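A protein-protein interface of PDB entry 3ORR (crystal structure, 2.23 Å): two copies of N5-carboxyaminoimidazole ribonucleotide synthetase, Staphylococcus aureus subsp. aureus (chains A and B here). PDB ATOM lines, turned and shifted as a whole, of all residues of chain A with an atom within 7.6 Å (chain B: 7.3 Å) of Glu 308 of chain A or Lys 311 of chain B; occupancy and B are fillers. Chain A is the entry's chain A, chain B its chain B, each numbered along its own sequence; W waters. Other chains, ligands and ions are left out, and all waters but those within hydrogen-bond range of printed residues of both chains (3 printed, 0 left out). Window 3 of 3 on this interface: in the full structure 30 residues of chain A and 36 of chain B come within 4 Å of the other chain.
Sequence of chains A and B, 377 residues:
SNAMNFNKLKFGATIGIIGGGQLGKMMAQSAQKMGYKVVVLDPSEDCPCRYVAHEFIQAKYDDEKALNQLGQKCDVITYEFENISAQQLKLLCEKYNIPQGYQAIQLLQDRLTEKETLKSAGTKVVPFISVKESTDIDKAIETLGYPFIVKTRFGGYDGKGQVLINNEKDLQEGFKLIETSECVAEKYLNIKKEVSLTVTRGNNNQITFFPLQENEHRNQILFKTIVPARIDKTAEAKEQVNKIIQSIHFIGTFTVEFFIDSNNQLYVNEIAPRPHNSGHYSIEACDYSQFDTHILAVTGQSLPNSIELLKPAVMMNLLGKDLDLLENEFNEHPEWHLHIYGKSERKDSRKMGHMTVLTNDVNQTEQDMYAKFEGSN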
ATOM      1  N   THR A 208      30.702  16.244   5.063  1.00  0.00           N
ATOM      2  CA  THR A 208      29.958  16.924   6.125  1.00  0.00           C
ATOM      3  C   THR A 208      30.298  18.411   6.134  1.00  0.00           C
ATOM      4  O   THR A 208      31.433  18.826   5.878  1.00  0.00           O
ATOM      5  CB  THR A 208      30.268  16.283   7.484  1.00  0.00           C
ATOM      6  OG1 THR A 208      30.065  14.869   7.341  1.00  0.00           O
ATOM      7  CG2 THR A 208      29.328  16.775   8.598  1.00  0.00           C
ATOM      8  N   PHE A 209      29.288  19.206   6.449  1.00  0.00           N
ATOM      9  CA  PHE A 209      29.380  20.633   6.385  1.00  0.00           C
ATOM     10  C   PHE A 209      29.369  21.301   7.767  1.00  0.00           C
ATOM     11  O   PHE A 209      28.543  20.972   8.618  1.00  0.00           O
ATOM     12  CB  PHE A 209      28.215  21.113   5.540  1.00  0.00           C
ATOM     13  CG  PHE A 209      28.396  20.852   4.080  1.00  0.00           C
ATOM     14  CD1 PHE A 209      29.210  21.684   3.311  1.00  0.00           C
ATOM     15  CD2 PHE A 209      27.741  19.785   3.464  1.00  0.00           C
ATOM     16  CE1 PHE A 209      29.384  21.457   1.936  1.00  0.00           C
ATOM     17  CE2 PHE A 209      27.895  19.541   2.094  1.00  0.00           C
ATOM     18  CZ  PHE A 209      28.715  20.391   1.330  1.00  0.00           C
ATOM     19  N   PHE A 210      30.271  22.246   8.011  1.00  0.00           N
ATOM     20  CA  PHE A 210      30.156  23.007   9.266  1.00  0.00           C
ATOM     21  C   PHE A 210      29.171  24.189   9.047  1.00  0.00           C
ATOM     22  O   PHE A 210      28.792  24.456   7.906  1.00  0.00           O
ATOM     23  CB  PHE A 210      31.528  23.487   9.749  1.00  0.00           C
ATOM     24  CG  PHE A 210      32.342  22.398  10.444  1.00  0.00           C
ATOM     25  CD1 PHE A 210      33.018  21.427   9.720  1.00  0.00           C
ATOM     26  CD2 PHE A 210      32.381  22.326  11.831  1.00  0.00           C
ATOM     27  CE1 PHE A 210      33.754  20.395  10.410  1.00  0.00           C
ATOM     28  CE2 PHE A 210      33.116  21.351  12.490  1.00  0.00           C
ATOM     29  CZ  PHE A 210      33.798  20.378  11.779  1.00  0.00           C
ATOM     30  N   PRO A 211      28.760  24.885  10.137  1.00  0.00           N
ATOM     31  CA  PRO A 211      27.893  26.060  10.002  1.00  0.00           C
ATOM     32  C   PRO A 211      28.545  27.169   9.203  1.00  0.00           C
ATOM     33  O   PRO A 211      29.714  27.504   9.431  1.00  0.00           O
ATOM     34  CB  PRO A 211      27.651  26.511  11.452  1.00  0.00           C
ATOM     35  CG  PRO A 211      27.925  25.207  12.294  1.00  0.00           C
ATOM     36  CD  PRO A 211      28.980  24.494  11.545  1.00  0.00           C
ATOM     37  N   TYR A 281      36.526  28.433  15.617  1.00  0.00           N
ATOM     38  CA  TYR A 281      35.401  28.578  16.526  1.00  0.00           C
ATOM     39  C   TYR A 281      34.819  27.195  16.890  1.00  0.00           C
ATOM     40  O   TYR A 281      34.262  27.000  17.958  1.00  0.00           O
ATOM     41  CB  TYR A 281      34.310  29.460  15.889  1.00  0.00           C
ATOM     42  CG  TYR A 281      33.550  28.708  14.832  1.00  0.00           C
ATOM     43  CD1 TYR A 281      34.013  28.665  13.526  1.00  0.00           C
ATOM     44  CD2 TYR A 281      32.420  27.984  15.147  1.00  0.00           C
ATOM     45  CE1 TYR A 281      33.370  27.915  12.566  1.00  0.00           C
ATOM     46  CE2 TYR A 281      31.765  27.241  14.199  1.00  0.00           C
ATOM     47  CZ  TYR A 281      32.260  27.201  12.899  1.00  0.00           C
ATOM     48  OH  TYR A 281      31.624  26.462  11.905  1.00  0.00           O
ATOM     49  N   SER A 282      34.890  26.266  15.955  1.00  0.00           N
ATOM     50  CA  SER A 282      34.202  24.978  16.065  1.00  0.00           C
ATOM     51  C   SER A 282      34.659  24.113  17.251  1.00  0.00           C
ATOM     52  O   SER A 282      33.910  23.236  17.733  1.00  0.00           O
ATOM     53  CB  SER A 282      34.366  24.202  14.746  1.00  0.00           C
ATOM     54  OG  SER A 282      35.724  23.854  14.554  1.00  0.00           O
ATOM     55  N   GLU A 284      34.962  25.039  20.316  1.00  0.00           N
ATOM     56  CA  GLU A 284      34.103  25.281  21.498  1.00  0.00           C
ATOM     57  C   GLU A 284      32.631  25.210  21.161  1.00  0.00           C
ATOM     58  O   GLU A 284      31.855  24.671  21.939  1.00  0.00           O
ATOM     59  CB  GLU A 284      34.378  26.653  22.120  1.00  0.00           C
ATOM     60  CG  GLU A 284      35.666  26.713  22.978  1.00  0.00           C
ATOM     61  CD  GLU A 284      36.920  26.904  22.126  1.00  0.00           C
ATOM     62  OE1 GLU A 284      36.838  27.354  20.962  1.00  0.00           O
ATOM     63  OE2 GLU A 284      38.011  26.574  22.606  1.00  0.00           O
ATOM     64  N   ALA A 285      32.260  25.672  19.980  1.00  0.00           N
ATOM     65  CA  ALA A 285      30.855  25.903  19.613  1.00  0.00           C
ATOM     66  C   ALA A 285      30.142  24.735  18.971  1.00  0.00           C
ATOM     67  O   ALA A 285      28.911  24.694  18.983  1.00  0.00           O
ATOM     68  CB  ALA A 285      30.767  27.118  18.712  1.00  0.00           C
ATOM     69  N   CYS A 286      30.894  23.768  18.434  1.00  0.00           N
ATOM     70  CA  CYS A 286      30.290  22.625  17.730  1.00  0.00           C
ATOM     71  C   CYS A 286      30.476  21.323  18.464  1.00  0.00           C
ATOM     72  O   CYS A 286      31.286  21.234  19.411  1.00  0.00           O
ATOM     73  CB  CYS A 286      30.856  22.486  16.316  1.00  0.00           C
ATOM     74  SG  CYS A 286      30.538  23.892  15.308  1.00  0.00           S
ATOM     75  N   ASP A 287      29.722  20.308  18.034  1.00  0.00           N
ATOM     76  CA  ASP A 287      29.860  19.010  18.642  1.00  0.00           C
ATOM     77  C   ASP A 287      31.028  18.230  18.053  1.00  0.00           C
ATOM     78  O   ASP A 287      31.357  17.154  18.542  1.00  0.00           O
ATOM     79  CB  ASP A 287      28.535  18.201  18.578  1.00  0.00           C
ATOM     80  CG  ASP A 287      27.972  18.094  17.186  1.00  0.00           C
ATOM     81  OD1 ASP A 287      28.505  18.746  16.260  1.00  0.00           O
ATOM     82  OD2 ASP A 287      26.989  17.345  17.021  1.00  0.00           O
ATOM     83  N   TYR A 288      31.607  18.738  16.968  1.00  0.00           N
ATOM     84  CA  TYR A 288      32.919  18.255  16.455  1.00  0.00           C
ATOM     85  C   TYR A 288      33.706  19.505  16.047  1.00  0.00           C
ATOM     86  O   TYR A 288      33.102  20.503  15.696  1.00  0.00           O
ATOM     87  CB  TYR A 288      32.765  17.344  15.230  1.00  0.00           C
ATOM     88  CG  TYR A 288      31.919  16.098  15.489  1.00  0.00           C
ATOM     89  CD1 TYR A 288      30.519  16.155  15.405  1.00  0.00           C
ATOM     90  CD2 TYR A 288      32.530  14.866  15.825  1.00  0.00           C
ATOM     91  CE1 TYR A 288      29.755  15.079  15.638  1.00  0.00           C
ATOM     92  CE2 TYR A 288      31.756  13.758  16.053  1.00  0.00           C
ATOM     93  CZ  TYR A 288      30.354  13.879  15.972  1.00  0.00           C
ATOM     94  OH  TYR A 288      29.544  12.800  16.141  1.00  0.00           O
ATOM     95  N   PRO A 304      30.658  12.231  11.029  1.00  0.00           N
ATOM     96  CA  PRO A 304      29.248  12.516  11.424  1.00  0.00           C
ATOM     97  C   PRO A 304      28.491  13.066  10.225  1.00  0.00           C
ATOM     98  O   PRO A 304      29.105  13.738   9.390  1.00  0.00           O
ATOM     99  CB  PRO A 304      29.394  13.596  12.485  1.00  0.00           C
ATOM    100  CG  PRO A 304      30.771  14.258  12.196  1.00  0.00           C
ATOM    101  CD  PRO A 304      31.634  13.140  11.641  1.00  0.00           C
ATOM    102  N   SER A 306      26.270  15.361  10.213  1.00  0.00           N
ATOM    103  CA  SER A 306      26.054  16.787  10.315  1.00  0.00           C
ATOM    104  C   SER A 306      26.818  17.287  11.521  1.00  0.00           C
ATOM    105  O   SER A 306      27.243  16.513  12.404  1.00  0.00           O
ATOM    106  CB  SER A 306      24.550  17.130  10.414  1.00  0.00           C
ATOM    107  OG  SER A 306      24.016  16.543  11.580  1.00  0.00           O
ATOM    108  N   ILE A 307      27.025  18.592  11.543  1.00  0.00           N
ATOM    109  CA  ILE A 307      27.698  19.183  12.633  1.00  0.00           C
ATOM    110  C   ILE A 307      26.675  20.094  13.246  1.00  0.00           C
ATOM    111  O   ILE A 307      25.903  20.727  12.546  1.00  0.00           O
ATOM    112  CB  ILE A 307      28.953  19.944  12.155  1.00  0.00           C
ATOM    113  CG1 ILE A 307      30.009  18.920  11.702  1.00  0.00           C
ATOM    114  CG2 ILE A 307      29.492  20.817  13.304  1.00  0.00           C
ATOM    115  CD1 ILE A 307      30.638  19.300  10.440  1.00  0.00           C
ATOM    116  N   GLU A 308      26.664  20.123  14.566  1.00  0.00           N
ATOM    117  CA  GLU A 308      25.694  20.889  15.295  1.00  0.00           C
ATOM    118  C   GLU A 308      26.394  22.069  15.926  1.00  0.00           C
ATOM    119  O   GLU A 308      27.441  21.924  16.552  1.00  0.00           O
ATOM    120  CB  GLU A 308      25.096  19.996  16.353  1.00  0.00           C
ATOM    121  CG  GLU A 308      23.855  20.520  17.013  1.00  0.00           C
ATOM    122  CD  GLU A 308      23.129  19.390  17.741  1.00  0.00           C
ATOM    123  OE1 GLU A 308      23.140  18.275  17.185  1.00  0.00           O
ATOM    124  OE2 GLU A 308      22.564  19.609  18.846  1.00  0.00           O
ATOM    125  N   LEU A 309      25.829  23.243  15.738  1.00  0.00           N
ATOM    126  CA  LEU A 309      26.313  24.427  16.400  1.00  0.00           C
ATOM    127  C   LEU A 309      25.617  24.457  17.773  1.00  0.00           C
ATOM    128  O   LEU A 309      24.394  24.806  17.884  1.00  0.00           O
ATOM    129  CB  LEU A 309      25.982  25.675  15.571  1.00  0.00           C
ATOM    130  CG  LEU A 309      26.366  27.021  16.142  1.00  0.00           C
ATOM    131  CD1 LEU A 309      27.907  27.167  16.148  1.00  0.00           C
ATOM    132  CD2 LEU A 309      25.678  28.168  15.289  1.00  0.00           C
ATOM    133  N   LEU A 310      26.369  24.073  18.799  1.00  0.00           N
ATOM    134  CA  LEU A 310      25.840  23.971  20.178  1.00  0.00           C
ATOM    135  C   LEU A 310      25.547  25.351  20.772  1.00  0.00           C
ATOM    136  O   LEU A 310      24.634  25.510  21.587  1.00  0.00           O
ATOM    137  CB  LEU A 310      26.798  23.173  21.086  1.00  0.00           C
ATOM    138  CG  LEU A 310      27.029  21.711  20.581  1.00  0.00           C
ATOM    139  CD1 LEU A 310      27.980  20.915  21.455  1.00  0.00           C
ATOM    140  CD2 LEU A 310      25.689  20.948  20.437  1.00  0.00           C
ATOM    141  N   LYS A 311      26.309  26.360  20.360  1.00  0.00           N
ATOM    142  CA  LYS A 311      26.048  27.717  20.793  1.00  0.00           C
ATOM    143  C   LYS A 311      26.714  28.714  19.833  1.00  0.00           C
ATOM    144  O   LYS A 311      27.803  28.432  19.321  1.00  0.00           O
ATOM    145  CB  LYS A 311      26.559  27.890  22.210  1.00  0.00           C
ATOM    146  CG  LYS A 311      26.051  29.154  22.884  1.00  0.00           C
ATOM    147  CD  LYS A 311      26.511  29.288  24.325  1.00  0.00           C
ATOM    148  CE  LYS A 311      26.157  30.704  24.853  1.00  0.00           C
ATOM    149  NZ  LYS A 311      26.340  30.707  26.325  1.00  0.00           N
ATOM    150  N   VAL B 227      24.382  12.639  32.319  1.00  0.00           N
ATOM    151  CA  VAL B 227      24.217  14.043  32.633  1.00  0.00           C
ATOM    152  C   VAL B 227      23.197  14.679  31.706  1.00  0.00           C
ATOM    153  O   VAL B 227      23.333  14.590  30.481  1.00  0.00           O
ATOM    154  CB  VAL B 227      25.599  14.800  32.495  1.00  0.00           C
ATOM    155  CG1 VAL B 227      25.512  16.213  33.060  1.00  0.00           C
ATOM    156  CG2 VAL B 227      26.730  13.974  33.173  1.00  0.00           C
ATOM    157  N   PRO B 228      22.188  15.371  32.272  1.00  0.00           N
ATOM    158  CA  PRO B 228      22.025  15.635  33.721  1.00  0.00           C
ATOM    159  C   PRO B 228      21.534  14.420  34.507  1.00  0.00           C
ATOM    160  O   PRO B 228      20.836  13.578  33.960  1.00  0.00           O
ATOM    161  CB  PRO B 228      20.993  16.775  33.776  1.00  0.00           C
ATOM    162  CG  PRO B 228      20.137  16.591  32.476  1.00  0.00           C
ATOM    163  CD  PRO B 228      21.063  15.887  31.448  1.00  0.00           C
ATOM    164  N   TYR B 281      32.927  13.726  30.717  1.00  0.00           N
ATOM    165  CA  TYR B 281      31.862  14.079  29.761  1.00  0.00           C
ATOM    166  C   TYR B 281      31.956  15.585  29.407  1.00  0.00           C
ATOM    167  O   TYR B 281      31.544  15.992  28.335  1.00  0.00           O
ATOM    168  CB  TYR B 281      30.456  13.802  30.345  1.00  0.00           C
ATOM    169  CG  TYR B 281      30.096  14.817  31.409  1.00  0.00           C
ATOM    170  CD1 TYR B 281      30.634  14.727  32.712  1.00  0.00           C
ATOM    171  CD2 TYR B 281      29.319  15.910  31.106  1.00  0.00           C
ATOM    172  CE1 TYR B 281      30.369  15.666  33.662  1.00  0.00           C
ATOM    173  CE2 TYR B 281      29.034  16.877  32.091  1.00  0.00           C
ATOM    174  CZ  TYR B 281      29.564  16.737  33.353  1.00  0.00           C
ATOM    175  OH  TYR B 281      29.295  17.701  34.312  1.00  0.00           O
ATOM    176  N   GLU B 284      33.119  17.387  25.978  1.00  0.00           N
ATOM    177  CA  GLU B 284      32.247  17.560  24.792  1.00  0.00           C
ATOM    178  C   GLU B 284      30.964  18.273  25.157  1.00  0.00           C
ATOM    179  O   GLU B 284      30.416  19.041  24.366  1.00  0.00           O
ATOM    180  CB  GLU B 284      31.893  16.208  24.128  1.00  0.00           C
ATOM    181  CG  GLU B 284      33.089  15.610  23.289  1.00  0.00           C
ATOM    182  CD  GLU B 284      34.113  14.872  24.109  1.00  0.00           C
ATOM    183  OE1 GLU B 284      33.821  14.548  25.281  1.00  0.00           O
ATOM    184  OE2 GLU B 284      35.234  14.611  23.576  1.00  0.00           O
ATOM    185  N   ALA B 285      30.497  18.055  26.383  1.00  0.00           N
ATOM    186  CA  ALA B 285      29.118  18.440  26.694  1.00  0.00           C
ATOM    187  C   ALA B 285      28.956  19.878  27.201  1.00  0.00           C
ATOM    188  O   ALA B 285      27.855  20.441  27.127  1.00  0.00           O
ATOM    189  CB  ALA B 285      28.528  17.474  27.658  1.00  0.00           C
ATOM    190  N   CYS B 286      30.026  20.470  27.724  1.00  0.00           N
ATOM    191  CA  CYS B 286      29.900  21.740  28.433  1.00  0.00           C
ATOM    192  C   CYS B 286      30.697  22.780  27.717  1.00  0.00           C
ATOM    193  O   CYS B 286      31.546  22.444  26.907  1.00  0.00           O
ATOM    194  CB  CYS B 286      30.452  21.610  29.866  1.00  0.00           C
ATOM    195  SG  CYS B 286      29.552  20.503  30.920  1.00  0.00           S
ATOM    196  N   ASP B 287      30.457  24.049  28.071  1.00  0.00           N
ATOM    197  CA  ASP B 287      31.219  25.145  27.504  1.00  0.00           C
ATOM    198  C   ASP B 287      32.651  25.240  28.036  1.00  0.00           C
ATOM    199  O   ASP B 287      33.492  25.854  27.393  1.00  0.00           O
ATOM    200  CB  ASP B 287      30.475  26.498  27.603  1.00  0.00           C
ATOM    201  CG  ASP B 287      29.957  26.816  29.011  1.00  0.00           C
ATOM    202  OD1 ASP B 287      30.206  26.044  29.961  1.00  0.00           O
ATOM    203  OD2 ASP B 287      29.306  27.875  29.169  1.00  0.00           O
ATOM    204  N   GLU B 308      27.765  25.727  31.698  1.00  0.00           N
ATOM    205  CA  GLU B 308      26.562  25.416  30.941  1.00  0.00           C
ATOM    206  C   GLU B 308      26.733  24.045  30.300  1.00  0.00           C
ATOM    207  O   GLU B 308      27.776  23.769  29.657  1.00  0.00           O
ATOM    208  CB  GLU B 308      26.404  26.443  29.842  1.00  0.00           C
ATOM    209  CG  GLU B 308      25.051  26.426  29.124  1.00  0.00           C
ATOM    210  CD  GLU B 308      24.797  27.738  28.350  1.00  0.00           C
ATOM    211  OE1 GLU B 308      25.278  28.810  28.840  1.00  0.00           O
ATOM    212  OE2 GLU B 308      24.120  27.683  27.281  1.00  0.00           O
ATOM    213  N   LEU B 309      25.733  23.194  30.503  1.00  0.00           N
ATOM    214  CA  LEU B 309      25.566  21.923  29.799  1.00  0.00           C
ATOM    215  C   LEU B 309      24.982  22.261  28.413  1.00  0.00           C
ATOM    216  O   LEU B 309      23.771  22.579  28.274  1.00  0.00           O
ATOM    217  CB  LEU B 309      24.581  21.016  30.566  1.00  0.00           C
ATOM    218  CG  LEU B 309      24.435  19.606  29.963  1.00  0.00           C
ATOM    219  CD1 LEU B 309      25.765  18.832  30.071  1.00  0.00           C
ATOM    220  CD2 LEU B 309      23.331  18.864  30.723  1.00  0.00           C
ATOM    221  N   LEU B 310      25.837  22.243  27.401  1.00  0.00           N
ATOM    222  CA  LEU B 310      25.437  22.557  26.034  1.00  0.00           C
ATOM    223  C   LEU B 310      24.575  21.445  25.417  1.00  0.00           C
ATOM    224  O   LEU B 310      23.744  21.698  24.535  1.00  0.00           O
ATOM    225  CB  LEU B 310      26.669  22.808  25.168  1.00  0.00           C
ATOM    226  CG  LEU B 310      27.514  24.009  25.594  1.00  0.00           C
ATOM    227  CD1 LEU B 310      28.853  24.170  24.800  1.00  0.00           C
ATOM    228  CD2 LEU B 310      26.682  25.309  25.546  1.00  0.00           C
ATOM    229  N   LYS B 311      24.786  20.204  25.871  1.00  0.00           N
ATOM    230  CA  LYS B 311      23.953  19.101  25.420  1.00  0.00           C
ATOM    231  C   LYS B 311      24.158  17.915  26.347  1.00  0.00           C
ATOM    232  O   LYS B 311      25.295  17.677  26.731  1.00  0.00           O
ATOM    233  CB  LYS B 311      24.346  18.692  23.991  1.00  0.00           C
ATOM    234  CG  LYS B 311      23.672  17.381  23.529  1.00  0.00           C
ATOM    235  CD  LYS B 311      24.017  17.074  22.098  1.00  0.00           C
ATOM    236  CE  LYS B 311      22.930  17.389  21.138  1.00  0.00           C
ATOM    237  NZ  LYS B 311      23.028  16.377  20.035  1.00  0.00           N
ATOM    238  N   PRO B 312      23.078  17.156  26.666  1.00  0.00           N
ATOM    239  CA  PRO B 312      23.184  15.991  27.559  1.00  0.00           C
ATOM    240  C   PRO B 312      24.129  14.941  27.036  1.00  0.00           C
ATOM    241  O   PRO B 312      24.382  14.874  25.850  1.00  0.00           O
ATOM    242  CB  PRO B 312      21.754  15.423  27.604  1.00  0.00           C
ATOM    243  CG  PRO B 312      20.850  16.617  27.304  1.00  0.00           C
ATOM    244  CD  PRO B 312      21.682  17.350  26.212  1.00  0.00           C
ATOM    245  N   ALA B 313      24.579  14.061  27.927  1.00  0.00           N
ATOM    246  CA  ALA B 313      25.646  13.148  27.569  1.00  0.00           C
ATOM    247  C   ALA B 313      25.578  11.858  28.325  1.00  0.00           C
ATOM    248  O   ALA B 313      25.225  11.840  29.499  1.00  0.00           O
ATOM    249  CB  ALA B 313      27.040  13.853  27.815  1.00  0.00           C
ATOM    250  N   VAL B 314      25.967  10.779  27.673  1.00  0.00           N
ATOM    251  CA  VAL B 314      26.182   9.508  28.357  1.00  0.00           C
ATOM    252  C   VAL B 314      27.623   9.131  28.100  1.00  0.00           C
ATOM    253  O   VAL B 314      28.006   8.962  26.963  1.00  0.00           O
ATOM    254  CB  VAL B 314      25.253   8.370  27.891  1.00  0.00           C
ATOM    255  CG1 VAL B 314      25.488   7.115  28.736  1.00  0.00           C
ATOM    256  CG2 VAL B 314      23.784   8.796  27.954  1.00  0.00           C
ATOM    257  N   VAL B 357      28.965  10.259  24.487  1.00  0.00           N
ATOM    258  CA  VAL B 357      27.933  10.346  23.480  1.00  0.00           C
ATOM    259  C   VAL B 357      27.015  11.474  23.858  1.00  0.00           C
ATOM    260  O   VAL B 357      26.362  11.397  24.872  1.00  0.00           O
ATOM    261  CB  VAL B 357      27.068   9.040  23.426  1.00  0.00           C
ATOM    262  CG1 VAL B 357      25.990   9.115  22.260  1.00  0.00           C
ATOM    263  CG2 VAL B 357      27.924   7.776  23.347  1.00  0.00           C
ATOM    264  N   LEU B 358      26.963  12.529  23.052  1.00  0.00           N
ATOM    265  CA  LEU B 358      26.029  13.606  23.259  1.00  0.00           C
ATOM    266  C   LEU B 358      24.688  13.082  22.731  1.00  0.00           C
ATOM    267  O   LEU B 358      24.646  12.424  21.705  1.00  0.00           O
ATOM    268  CB  LEU B 358      26.468  14.832  22.464  1.00  0.00           C
ATOM    269  CG  LEU B 358      27.890  15.416  22.713  1.00  0.00           C
ATOM    270  CD1 LEU B 358      28.048  16.725  21.969  1.00  0.00           C
ATOM    271  CD2 LEU B 358      28.109  15.637  24.203  1.00  0.00           C
ATOM    272  N   THR B 359      23.604  13.370  23.434  1.00  0.00           N
ATOM    273  CA  THR B 359      22.299  12.883  23.027  1.00  0.00           C
ATOM    274  C   THR B 359      21.231  13.847  23.507  1.00  0.00           C
ATOM    275  O   THR B 359      21.428  14.560  24.501  1.00  0.00           O
ATOM    276  CB  THR B 359      22.043  11.464  23.595  1.00  0.00           C
ATOM    277  OG1 THR B 359      20.702  11.052  23.295  1.00  0.00           O
ATOM    278  CG2 THR B 359      22.277  11.431  25.133  1.00  0.00           C
ATOM    279  N   ASN B 360      20.098  13.869  22.797  1.00  0.00           N
ATOM    280  CA  ASN B 360      18.936  14.575  23.248  1.00  0.00           C
ATOM    281  C   ASN B 360      17.937  13.613  23.865  1.00  0.00           C
ATOM    282  O   ASN B 360      16.790  13.995  24.180  1.00  0.00           O
ATOM    283  CB  ASN B 360      18.292  15.321  22.068  1.00  0.00           C
ATOM    284  CG  ASN B 360      19.106  16.541  21.654  1.00  0.00           C
ATOM    285  OD1 ASN B 360      19.414  17.372  22.487  1.00  0.00           O
ATOM    286  ND2 ASN B 360      19.443  16.643  20.392  1.00  0.00           N
ATOM    287  N   VAL B 362      18.670  10.860  26.734  1.00  0.00           N
ATOM    288  CA  VAL B 362      19.544  10.125  27.637  1.00  0.00           C
ATOM    289  C   VAL B 362      19.023   8.696  27.857  1.00  0.00           C
ATOM    290  O   VAL B 362      19.768   7.715  27.721  1.00  0.00           O
ATOM    291  CB  VAL B 362      19.712  10.922  28.991  1.00  0.00           C
ATOM    292  CG1 VAL B 362      20.034   9.997  30.127  1.00  0.00           C
ATOM    293  CG2 VAL B 362      20.794  12.003  28.827  1.00  0.00           C
HETATM  294  O   HOH W   1      28.637  29.548  27.292  1.00  0.00           O
HETATM  295  O   HOH W   2      25.613  16.334  18.851  1.00  0.00           O
HETATM  296  O   HOH W   3      31.966  19.115  21.610  1.00  0.00           O
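The side-chain carboxylate (OE1) of Glu 308 of chain A is in salt-bridge range of the side-chain amino group (NZ) of Lys 311 of chain B, 3.4 Å away.
NZ of Lys 311 of chain A lies within salt-bridge range of OE1 of Glu 308 of chain B, at 3.3 Å.
Water W2 bridges OD2 of Asp 287 of chain A (2.5 Å) and NZ of Lys 311 of chain B (2.8 Å).
Water W1 bridges the side-chain carboxylate of Asp 287 of chain B and the side-chain amino group of Lys 311 of chain A.
Water W3 bridges O of Cys 286 of chain A (3.1 Å) and O of Glu 284 of chain B (3.2 Å).
Glu 308 of chain A touches Lys 311 of chain B, and with the chains exchanged Lys 311 of chain A touches Glu 308 of chain B.
9 positions are printed for both chains.
The backbone NH of Lys 311 of chain A sits at hydrogen-bond distance from the backbone carbonyl oxygen of Ala 285 of chain A (3.4 Å).
The side-chain carboxylate (OD1) of Asp 287 of chain A lies within hydrogen-bond range of the backbone NH (N) of Glu 308 of chain A.
The backbone carbonyl oxygen (O) of Ala 285 of chain B is in hydrogen-bond range of the backbone NH (N) of Lys 311 of chain B, at 3.3 Å.
OD1 of Asp 287 of chain B is in hydrogen-bond range of N of Glu 308 of chain B, at 3.0 Å.
Pro 211 of chain A touches none of the printed residues of chain B.
Of the printed residues of chain B, Asp 287 of chain A touches Leu 358 (3.7 Å).
Glu 308 of chain A touches one residue of chain B.
Of the printed residues of chain B, Lys 311 of chain A touches Glu 308.
Of the printed residues of chain A, Glu 308 of chain B touches Lys 311.
Of the printed residues of chain A, Lys 311 of chain B touches Glu 308.
Printed residues of chain A within 4 Å of Leu 358 of chain B: Asp 287.
Asn 360 of chain B touches none of the printed residues of chain A.
The nearest residue of chain B that does not touch Glu 308 of chain A is Asn 360 of chain B (4.6 Å).
The nearest residue of chain A that does not touch Lys 311 of chain B is Leu 310 of chain A (4.4 Å).
Of the 19 printed residues of chain B, 3 touch a printed residue of chain A.
Printed residues of chain B that touch a printed residue of chain A: Glu 308, Lys 311 and Leu 358.
Among the printed residues, Asp or Glu carboxylates within 4 Å of a Lys or Arg side-chain nitrogen of the other chain: Glu 308 of chain A with Lys 311 of chain B and Lys 311 of chain A with Glu 308 of chain B.
Among the printed residues, merely in contact across the chains: Asp 287 of chain A with Leu 358 of chain B.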
